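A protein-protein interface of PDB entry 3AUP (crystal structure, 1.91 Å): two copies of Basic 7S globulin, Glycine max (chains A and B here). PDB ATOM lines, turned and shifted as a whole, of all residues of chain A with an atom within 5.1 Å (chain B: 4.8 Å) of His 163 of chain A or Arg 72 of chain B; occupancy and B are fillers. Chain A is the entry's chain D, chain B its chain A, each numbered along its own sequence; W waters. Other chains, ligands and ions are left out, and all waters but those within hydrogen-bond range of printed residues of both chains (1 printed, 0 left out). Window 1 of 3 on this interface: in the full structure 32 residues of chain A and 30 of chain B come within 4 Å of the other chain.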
ATOM      1  N   LEU A 161     -18.246   4.422 -12.775  1.00  0.00           N
ATOM      2  CA  LEU A 161     -18.135   2.969 -12.816  1.00  0.00           C
ATOM      3  C   LEU A 161     -16.774   2.509 -12.338  1.00  0.00           C
ATOM      4  O   LEU A 161     -16.391   1.344 -12.573  1.00  0.00           O
ATOM      5  CB  LEU A 161     -18.321   2.436 -14.237  1.00  0.00           C
ATOM      6  CG  LEU A 161     -19.530   2.949 -15.014  1.00  0.00           C
ATOM      7  CD1 LEU A 161     -19.589   2.250 -16.377  1.00  0.00           C
ATOM      8  CD2 LEU A 161     -20.844   2.760 -14.313  1.00  0.00           C
ATOM      9  N   GLY A 162     -16.066   3.436 -11.682  1.00  0.00           N
ATOM     10  CA  GLY A 162     -14.722   3.209 -11.116  1.00  0.00           C
ATOM     11  C   GLY A 162     -14.764   2.205  -9.970  1.00  0.00           C
ATOM     12  O   GLY A 162     -15.825   1.836  -9.468  1.00  0.00           O
ATOM     13  N   HIS A 163     -13.597   1.706  -9.596  1.00  0.00           N
ATOM     14  CA  HIS A 163     -13.537   0.714  -8.582  1.00  0.00           C
ATOM     15  C   HIS A 163     -13.326   1.435  -7.283  1.00  0.00           C
ATOM     16  O   HIS A 163     -12.203   1.589  -6.811  1.00  0.00           O
ATOM     17  CB  HIS A 163     -12.405  -0.265  -8.797  1.00  0.00           C
ATOM     18  CG  HIS A 163     -12.395  -1.360  -7.794  1.00  0.00           C
ATOM     19  ND1 HIS A 163     -13.312  -2.384  -7.804  1.00  0.00           N
ATOM     20  CD2 HIS A 163     -11.610  -1.574  -6.719  1.00  0.00           C
ATOM     21  CE1 HIS A 163     -13.074  -3.199  -6.796  1.00  0.00           C
ATOM     22  NE2 HIS A 163     -12.052  -2.728  -6.117  1.00  0.00           N
ATOM     23  N   ALA A 164     -14.453   1.821  -6.722  1.00  0.00           N
ATOM     24  CA  ALA A 164     -14.550   2.643  -5.574  1.00  0.00           C
ATOM     25  C   ALA A 164     -15.841   2.206  -4.872  1.00  0.00           C
ATOM     26  O   ALA A 164     -16.774   1.687  -5.528  1.00  0.00           O
ATOM     27  CB  ALA A 164     -14.604   4.133  -6.010  1.00  0.00           C
ATOM     28  N   PRO A 165     -15.905   2.398  -3.549  1.00  0.00           N
ATOM     29  CA  PRO A 165     -16.922   1.715  -2.739  1.00  0.00           C
ATOM     30  C   PRO A 165     -18.375   2.018  -3.102  1.00  0.00           C
ATOM     31  O   PRO A 165     -19.226   1.194  -2.898  1.00  0.00           O
ATOM     32  CB  PRO A 165     -16.619   2.178  -1.329  1.00  0.00           C
ATOM     33  CG  PRO A 165     -15.710   3.262  -1.445  1.00  0.00           C
ATOM     34  CD  PRO A 165     -14.980   3.173  -2.717  1.00  0.00           C
ATOM     35  N   SER A 167     -19.325   3.234  -6.287  1.00  0.00           N
ATOM     36  CA  SER A 167     -19.515   3.316  -7.727  1.00  0.00           C
ATOM     37  C   SER A 167     -20.712   2.489  -8.170  1.00  0.00           C
ATOM     38  O   SER A 167     -21.244   1.682  -7.407  1.00  0.00           O
ATOM     39  CB  SER A 167     -18.282   2.840  -8.457  1.00  0.00           C
ATOM     40  OG  SER A 167     -18.118   1.428  -8.276  1.00  0.00           O
ATOM     41  N   ASN A 170     -20.227  -1.432  -8.012  1.00  0.00           N
ATOM     42  CA  ASN A 170     -20.092  -1.969  -6.691  1.00  0.00           C
ATOM     43  C   ASN A 170     -21.398  -1.986  -5.958  1.00  0.00           C
ATOM     44  O   ASN A 170     -21.706  -3.001  -5.358  1.00  0.00           O
ATOM     45  CB  ASN A 170     -18.949  -1.291  -5.933  1.00  0.00           C
ATOM     46  CG  ASN A 170     -17.621  -1.740  -6.454  1.00  0.00           C
ATOM     47  OD1 ASN A 170     -17.424  -2.950  -6.709  1.00  0.00           O
ATOM     48  ND2 ASN A 170     -16.707  -0.805  -6.670  1.00  0.00           N
ATOM     49  N   ARG A 180     -18.752  -9.954  -9.185  1.00  0.00           N
ATOM     50  CA  ARG A 180     -18.129  -8.633  -9.158  1.00  0.00           C
ATOM     51  C   ARG A 180     -17.465  -8.308 -10.465  1.00  0.00           C
ATOM     52  O   ARG A 180     -16.229  -8.326 -10.564  1.00  0.00           O
ATOM     53  CB  ARG A 180     -17.039  -8.591  -8.079  1.00  0.00           C
ATOM     54  CG  ARG A 180     -17.517  -8.111  -6.791  1.00  0.00           C
ATOM     55  CD  ARG A 180     -17.381  -6.586  -6.724  1.00  0.00           C
ATOM     56  NE  ARG A 180     -17.152  -6.186  -5.334  1.00  0.00           N
ATOM     57  CZ  ARG A 180     -18.045  -6.333  -4.358  1.00  0.00           C
ATOM     58  NH1 ARG A 180     -19.238  -6.894  -4.583  1.00  0.00           N
ATOM     59  NH2 ARG A 180     -17.746  -5.925  -3.143  1.00  0.00           N
ATOM     60  N   ILE A 224      -5.676  -0.648 -10.124  1.00  0.00           N
ATOM     61  CA  ILE A 224      -6.475   0.518  -9.837  1.00  0.00           C
ATOM     62  C   ILE A 224      -5.550   1.546  -9.329  1.00  0.00           C
ATOM     63  O   ILE A 224      -4.709   1.305  -8.424  1.00  0.00           O
ATOM     64  CB  ILE A 224      -7.519   0.208  -8.771  1.00  0.00           C
ATOM     65  CG1 ILE A 224      -8.339  -1.016  -9.198  1.00  0.00           C
ATOM     66  CG2 ILE A 224      -8.309   1.449  -8.383  1.00  0.00           C
ATOM     67  CD1 ILE A 224      -9.035  -0.919 -10.543  1.00  0.00           C
ATOM     68  N   GLY A 228      -8.453   6.163  -8.488  1.00  0.00           N
ATOM     69  CA  GLY A 228      -9.637   5.321  -8.754  1.00  0.00           C
ATOM     70  C   GLY A 228      -9.831   4.901 -10.201  1.00  0.00           C
ATOM     71  O   GLY A 228     -10.900   4.460 -10.594  1.00  0.00           O
ATOM     72  N   TYR A 230      -8.979   2.705 -13.658  1.00  0.00           N
ATOM     73  CA  TYR A 230      -8.556   1.425 -14.213  1.00  0.00           C
ATOM     74  C   TYR A 230      -7.288   1.624 -15.008  1.00  0.00           C
ATOM     75  O   TYR A 230      -7.197   2.568 -15.803  1.00  0.00           O
ATOM     76  CB  TYR A 230      -9.660   0.880 -15.115  1.00  0.00           C
ATOM     77  CG  TYR A 230     -10.921   0.546 -14.356  1.00  0.00           C
ATOM     78  CD1 TYR A 230     -10.922  -0.451 -13.398  1.00  0.00           C
ATOM     79  CD2 TYR A 230     -12.105   1.212 -14.595  1.00  0.00           C
ATOM     80  CE1 TYR A 230     -12.083  -0.773 -12.680  1.00  0.00           C
ATOM     81  CE2 TYR A 230     -13.253   0.906 -13.897  1.00  0.00           C
ATOM     82  CZ  TYR A 230     -13.237  -0.096 -12.937  1.00  0.00           C
ATOM     83  OH  TYR A 230     -14.371  -0.399 -12.238  1.00  0.00           O
ATOM     84  N   LEU A 375     -13.583  -7.433 -11.603  1.00  0.00           N
ATOM     85  CA  LEU A 375     -13.135  -6.844 -10.342  1.00  0.00           C
ATOM     86  C   LEU A 375     -12.877  -7.890  -9.265  1.00  0.00           C
ATOM     87  O   LEU A 375     -12.198  -7.602  -8.269  1.00  0.00           O
ATOM     88  CB  LEU A 375     -14.173  -5.818  -9.819  1.00  0.00           C
ATOM     89  CG  LEU A 375     -14.795  -4.744 -10.734  1.00  0.00           C
ATOM     90  CD1 LEU A 375     -15.619  -5.418 -11.759  1.00  0.00           C
ATOM     91  CD2 LEU A 375     -15.691  -3.731  -9.996  1.00  0.00           C
ATOM     92  N   THR B  68      -7.583  -4.868  -7.974  1.00  0.00           N
ATOM     93  CA  THR B  68      -8.903  -4.572  -7.450  1.00  0.00           C
ATOM     94  C   THR B  68      -9.124  -5.080  -6.045  1.00  0.00           C
ATOM     95  O   THR B  68      -9.778  -4.403  -5.251  1.00  0.00           O
ATOM     96  CB  THR B  68     -10.002  -5.153  -8.379  1.00  0.00           C
ATOM     97  OG1 THR B  68      -9.751  -6.546  -8.542  1.00  0.00           O
ATOM     98  CG2 THR B  68      -9.972  -4.417  -9.744  1.00  0.00           C
ATOM     99  N   GLN B  69      -8.618  -6.277  -5.709  1.00  0.00           N
ATOM    100  CA  GLN B  69      -8.790  -6.774  -4.332  1.00  0.00           C
ATOM    101  C   GLN B  69      -8.052  -5.896  -3.316  1.00  0.00           C
ATOM    102  O   GLN B  69      -8.614  -5.537  -2.280  1.00  0.00           O
ATOM    103  CB  GLN B  69      -8.356  -8.241  -4.166  1.00  0.00           C
ATOM    104  CG  GLN B  69      -9.046  -9.265  -5.099  1.00  0.00           C
ATOM    105  CD  GLN B  69      -8.156  -9.709  -6.254  1.00  0.00           C
ATOM    106  OE1 GLN B  69      -7.385  -8.895  -6.796  1.00  0.00           O
ATOM    107  NE2 GLN B  69      -8.229 -11.013  -6.633  1.00  0.00           N
ATOM    108  N   CYS B  70      -6.842  -5.455  -3.645  1.00  0.00           N
ATOM    109  CA  CYS B  70      -6.127  -4.564  -2.725  1.00  0.00           C
ATOM    110  C   CYS B  70      -6.856  -3.227  -2.617  1.00  0.00           C
ATOM    111  O   CYS B  70      -7.045  -2.739  -1.536  1.00  0.00           O
ATOM    112  CB  CYS B  70      -4.666  -4.405  -3.163  1.00  0.00           C
ATOM    113  SG  CYS B  70      -3.996  -6.053  -3.139  1.00  0.00           S
ATOM    114  N   SER B  71      -7.327  -2.681  -3.743  1.00  0.00           N
ATOM    115  CA  SER B  71      -8.150  -1.437  -3.727  1.00  0.00           C
ATOM    116  C   SER B  71      -9.394  -1.609  -2.840  1.00  0.00           C
ATOM    117  O   SER B  71      -9.752  -0.744  -2.017  1.00  0.00           O
ATOM    118  CB  SER B  71      -8.594  -1.028  -5.166  1.00  0.00           C
ATOM    119  OG  SER B  71      -9.380   0.175  -5.092  1.00  0.00           O
ATOM    120  N   ARG B  72     -10.064  -2.740  -2.972  1.00  0.00           N
ATOM    121  CA  ARG B  72     -11.283  -2.985  -2.166  1.00  0.00           C
ATOM    122  C   ARG B  72     -10.914  -3.033  -0.711  1.00  0.00           C
ATOM    123  O   ARG B  72     -11.585  -2.452   0.140  1.00  0.00           O
ATOM    124  CB  ARG B  72     -11.951  -4.309  -2.554  1.00  0.00           C
ATOM    125  CG  ARG B  72     -13.230  -4.569  -1.790  1.00  0.00           C
ATOM    126  CD  ARG B  72     -13.820  -5.860  -2.336  1.00  0.00           C
ATOM    127  NE  ARG B  72     -15.014  -6.237  -1.610  1.00  0.00           N
ATOM    128  CZ  ARG B  72     -15.509  -7.463  -1.572  1.00  0.00           C
ATOM    129  NH1 ARG B  72     -14.883  -8.469  -2.185  1.00  0.00           N
ATOM    130  NH2 ARG B  72     -16.617  -7.669  -0.906  1.00  0.00           N
ATOM    131  N   ALA B  73      -9.830  -3.735  -0.417  1.00  0.00           N
ATOM    132  CA  ALA B  73      -9.278  -3.742   0.960  1.00  0.00           C
ATOM    133  C   ALA B  73      -8.691  -2.396   1.428  1.00  0.00           C
ATOM    134  O   ALA B  73      -8.253  -2.290   2.567  1.00  0.00           O
ATOM    135  CB  ALA B  73      -8.223  -4.826   1.083  1.00  0.00           C
ATOM    136  N   ASN B  74      -8.648  -1.389   0.562  1.00  0.00           N
ATOM    137  CA  ASN B  74      -8.092  -0.081   0.910  1.00  0.00           C
ATOM    138  C   ASN B  74      -6.598  -0.109   1.281  1.00  0.00           C
ATOM    139  O   ASN B  74      -6.164   0.535   2.234  1.00  0.00           O
ATOM    140  CB  ASN B  74      -8.889   0.540   2.060  1.00  0.00           C
ATOM    141  CG  ASN B  74      -8.859   2.040   2.038  1.00  0.00           C
ATOM    142  OD1 ASN B  74      -8.578   2.684   3.065  1.00  0.00           O
ATOM    143  ND2 ASN B  74      -9.159   2.620   0.876  1.00  0.00           N
ATOM    144  N   LEU B 138     -11.860 -12.494   1.135  1.00  0.00           N
ATOM    145  CA  LEU B 138     -10.675 -11.730   1.397  1.00  0.00           C
ATOM    146  C   LEU B 138     -10.392 -11.668   2.912  1.00  0.00           C
ATOM    147  O   LEU B 138     -11.296 -11.483   3.740  1.00  0.00           O
ATOM    148  CB  LEU B 138     -10.832 -10.292   0.824  1.00  0.00           C
ATOM    149  CG  LEU B 138     -10.767 -10.010  -0.684  1.00  0.00           C
ATOM    150  CD1 LEU B 138     -11.204  -8.485  -1.040  1.00  0.00           C
ATOM    151  CD2 LEU B 138      -9.364 -10.370  -1.208  1.00  0.00           C
ATOM    152  N   PRO B 165     -14.588  -2.226   4.508  1.00  0.00           N
ATOM    153  CA  PRO B 165     -15.046  -2.791   3.231  1.00  0.00           C
ATOM    154  C   PRO B 165     -14.851  -4.303   3.089  1.00  0.00           C
ATOM    155  O   PRO B 165     -15.582  -4.908   2.344  1.00  0.00           O
ATOM    156  CB  PRO B 165     -14.218  -2.020   2.171  1.00  0.00           C
ATOM    157  CG  PRO B 165     -13.040  -1.432   2.942  1.00  0.00           C
ATOM    158  CD  PRO B 165     -13.606  -1.141   4.312  1.00  0.00           C
ATOM    159  N   ILE B 166     -13.932  -4.921   3.830  1.00  0.00           N
ATOM    160  CA  ILE B 166     -13.769  -6.369   3.747  1.00  0.00           C
ATOM    161  C   ILE B 166     -14.096  -7.099   5.055  1.00  0.00           C
ATOM    162  O   ILE B 166     -13.773  -8.231   5.216  1.00  0.00           O
ATOM    163  CB  ILE B 166     -12.437  -6.785   3.125  1.00  0.00           C
ATOM    164  CG1 ILE B 166     -11.244  -6.450   4.036  1.00  0.00           C
ATOM    165  CG2 ILE B 166     -12.306  -6.143   1.731  1.00  0.00           C
ATOM    166  CD1 ILE B 166      -9.994  -7.177   3.566  1.00  0.00           C
ATOM    167  N   GLN B 171     -18.732  -8.333   3.444  1.00  0.00           N
ATOM    168  CA  GLN B 171     -18.348  -9.298   2.392  1.00  0.00           C
ATOM    169  C   GLN B 171     -19.464 -10.304   2.171  1.00  0.00           C
ATOM    170  O   GLN B 171     -19.706 -10.676   1.025  1.00  0.00           O
ATOM    171  CB  GLN B 171     -17.090 -10.071   2.682  1.00  0.00           C
ATOM    172  CG  GLN B 171     -15.803  -9.383   2.238  1.00  0.00           C
ATOM    173  CD  GLN B 171     -14.646 -10.309   2.196  1.00  0.00           C
ATOM    174  OE1 GLN B 171     -14.490 -11.069   1.228  1.00  0.00           O
ATOM    175  NE2 GLN B 171     -13.793 -10.282   3.260  1.00  0.00           N
ATOM    176  N   SER B 174     -22.662  -8.562   0.470  1.00  0.00           N
ATOM    177  CA  SER B 174     -22.314  -8.278  -0.908  1.00  0.00           C
ATOM    178  C   SER B 174     -22.311  -9.482  -1.821  1.00  0.00           C
ATOM    179  O   SER B 174     -22.766  -9.404  -2.958  1.00  0.00           O
ATOM    180  CB  SER B 174     -20.939  -7.630  -0.954  1.00  0.00           C
ATOM    181  OG  SER B 174     -21.058  -6.313  -0.481  1.00  0.00           O
HETATM  182  O   HOH W   1     -21.196  -9.388  -5.141  1.00  0.00           O
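NE2 of His 163 of chain A sits at hydrogen-bond distance from O of Thr 68 of chain B, 3.0 Å away.
OG1 of Thr 68 of chain B lies within hydrogen-bond range of O of Leu 375 of chain A (2.7 Å).
NH2 of Arg 180 of chain A sits close to NH2 of Arg 72 of chain B, at 3.1 Å.
OH of Tyr 230 of chain A sits at hydrogen-bond distance from N of His 163 of chain A.
The backbone NH (N) of Leu 375 of chain A lies within hydrogen-bond range of the backbone carbonyl oxygen (O) of Arg 180 of chain A, 3.0 Å away.
Among the printed residues, merely in contact across the chains: His 163 of chain A with Ser 71 of chain B (3.3 Å), His 163 of chain A with Arg 72 of chain B (3.7 Å), Ile 224 of chain A with Thr 68 of chain B (3.7 Å) and Ile 224 of chain A with Ser 71 of chain B (3.7 Å).
His 163 of chain A touches just these residues of chain B: Thr 68 (3.0 Å), Ser 71 (3.3 Å) and Arg 72 (3.7 Å).
Of the printed residues of chain A, Arg 72 of chain B touches His 163 and Arg 180.
Of the printed residues of chain A, Ser 71 of chain B touches His 163 (3.3 Å) and Ile 224 (3.7 Å).
Printed residues of chain B within 4 Å of Arg 180 of chain A: Arg 72.
Printed residues of chain B within 4 Å of Leu 375 of chain A: Thr 68 (2.7 Å).
Of the printed residues of chain A, Thr 68 of chain B touches His 163, Ile 224 and Leu 375.
Of the printed residues of chain B, Ile 224 of chain A touches Thr 68 and Ser 71.
Gln 69 of chain B touches none of the printed residues of chain A.
The nearest printed residue of chain B that does not touch His 163 of chain A is Gln 69 of chain B (5.0 Å).
The nearest printed residue of chain B that does not touch Leu 375 of chain A is Gln 69 of chain B (4.6 Å).
Of the 12 printed residues of chain A, 4 touch a printed residue of chain B.
Among the printed residues, 7 pairs touch across the chains.
Position printed for both chains: 165.
Water W1 lies within hydrogen-bond range of O of Ser 174 of chain B and NH1 of Arg 180 of chain A.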
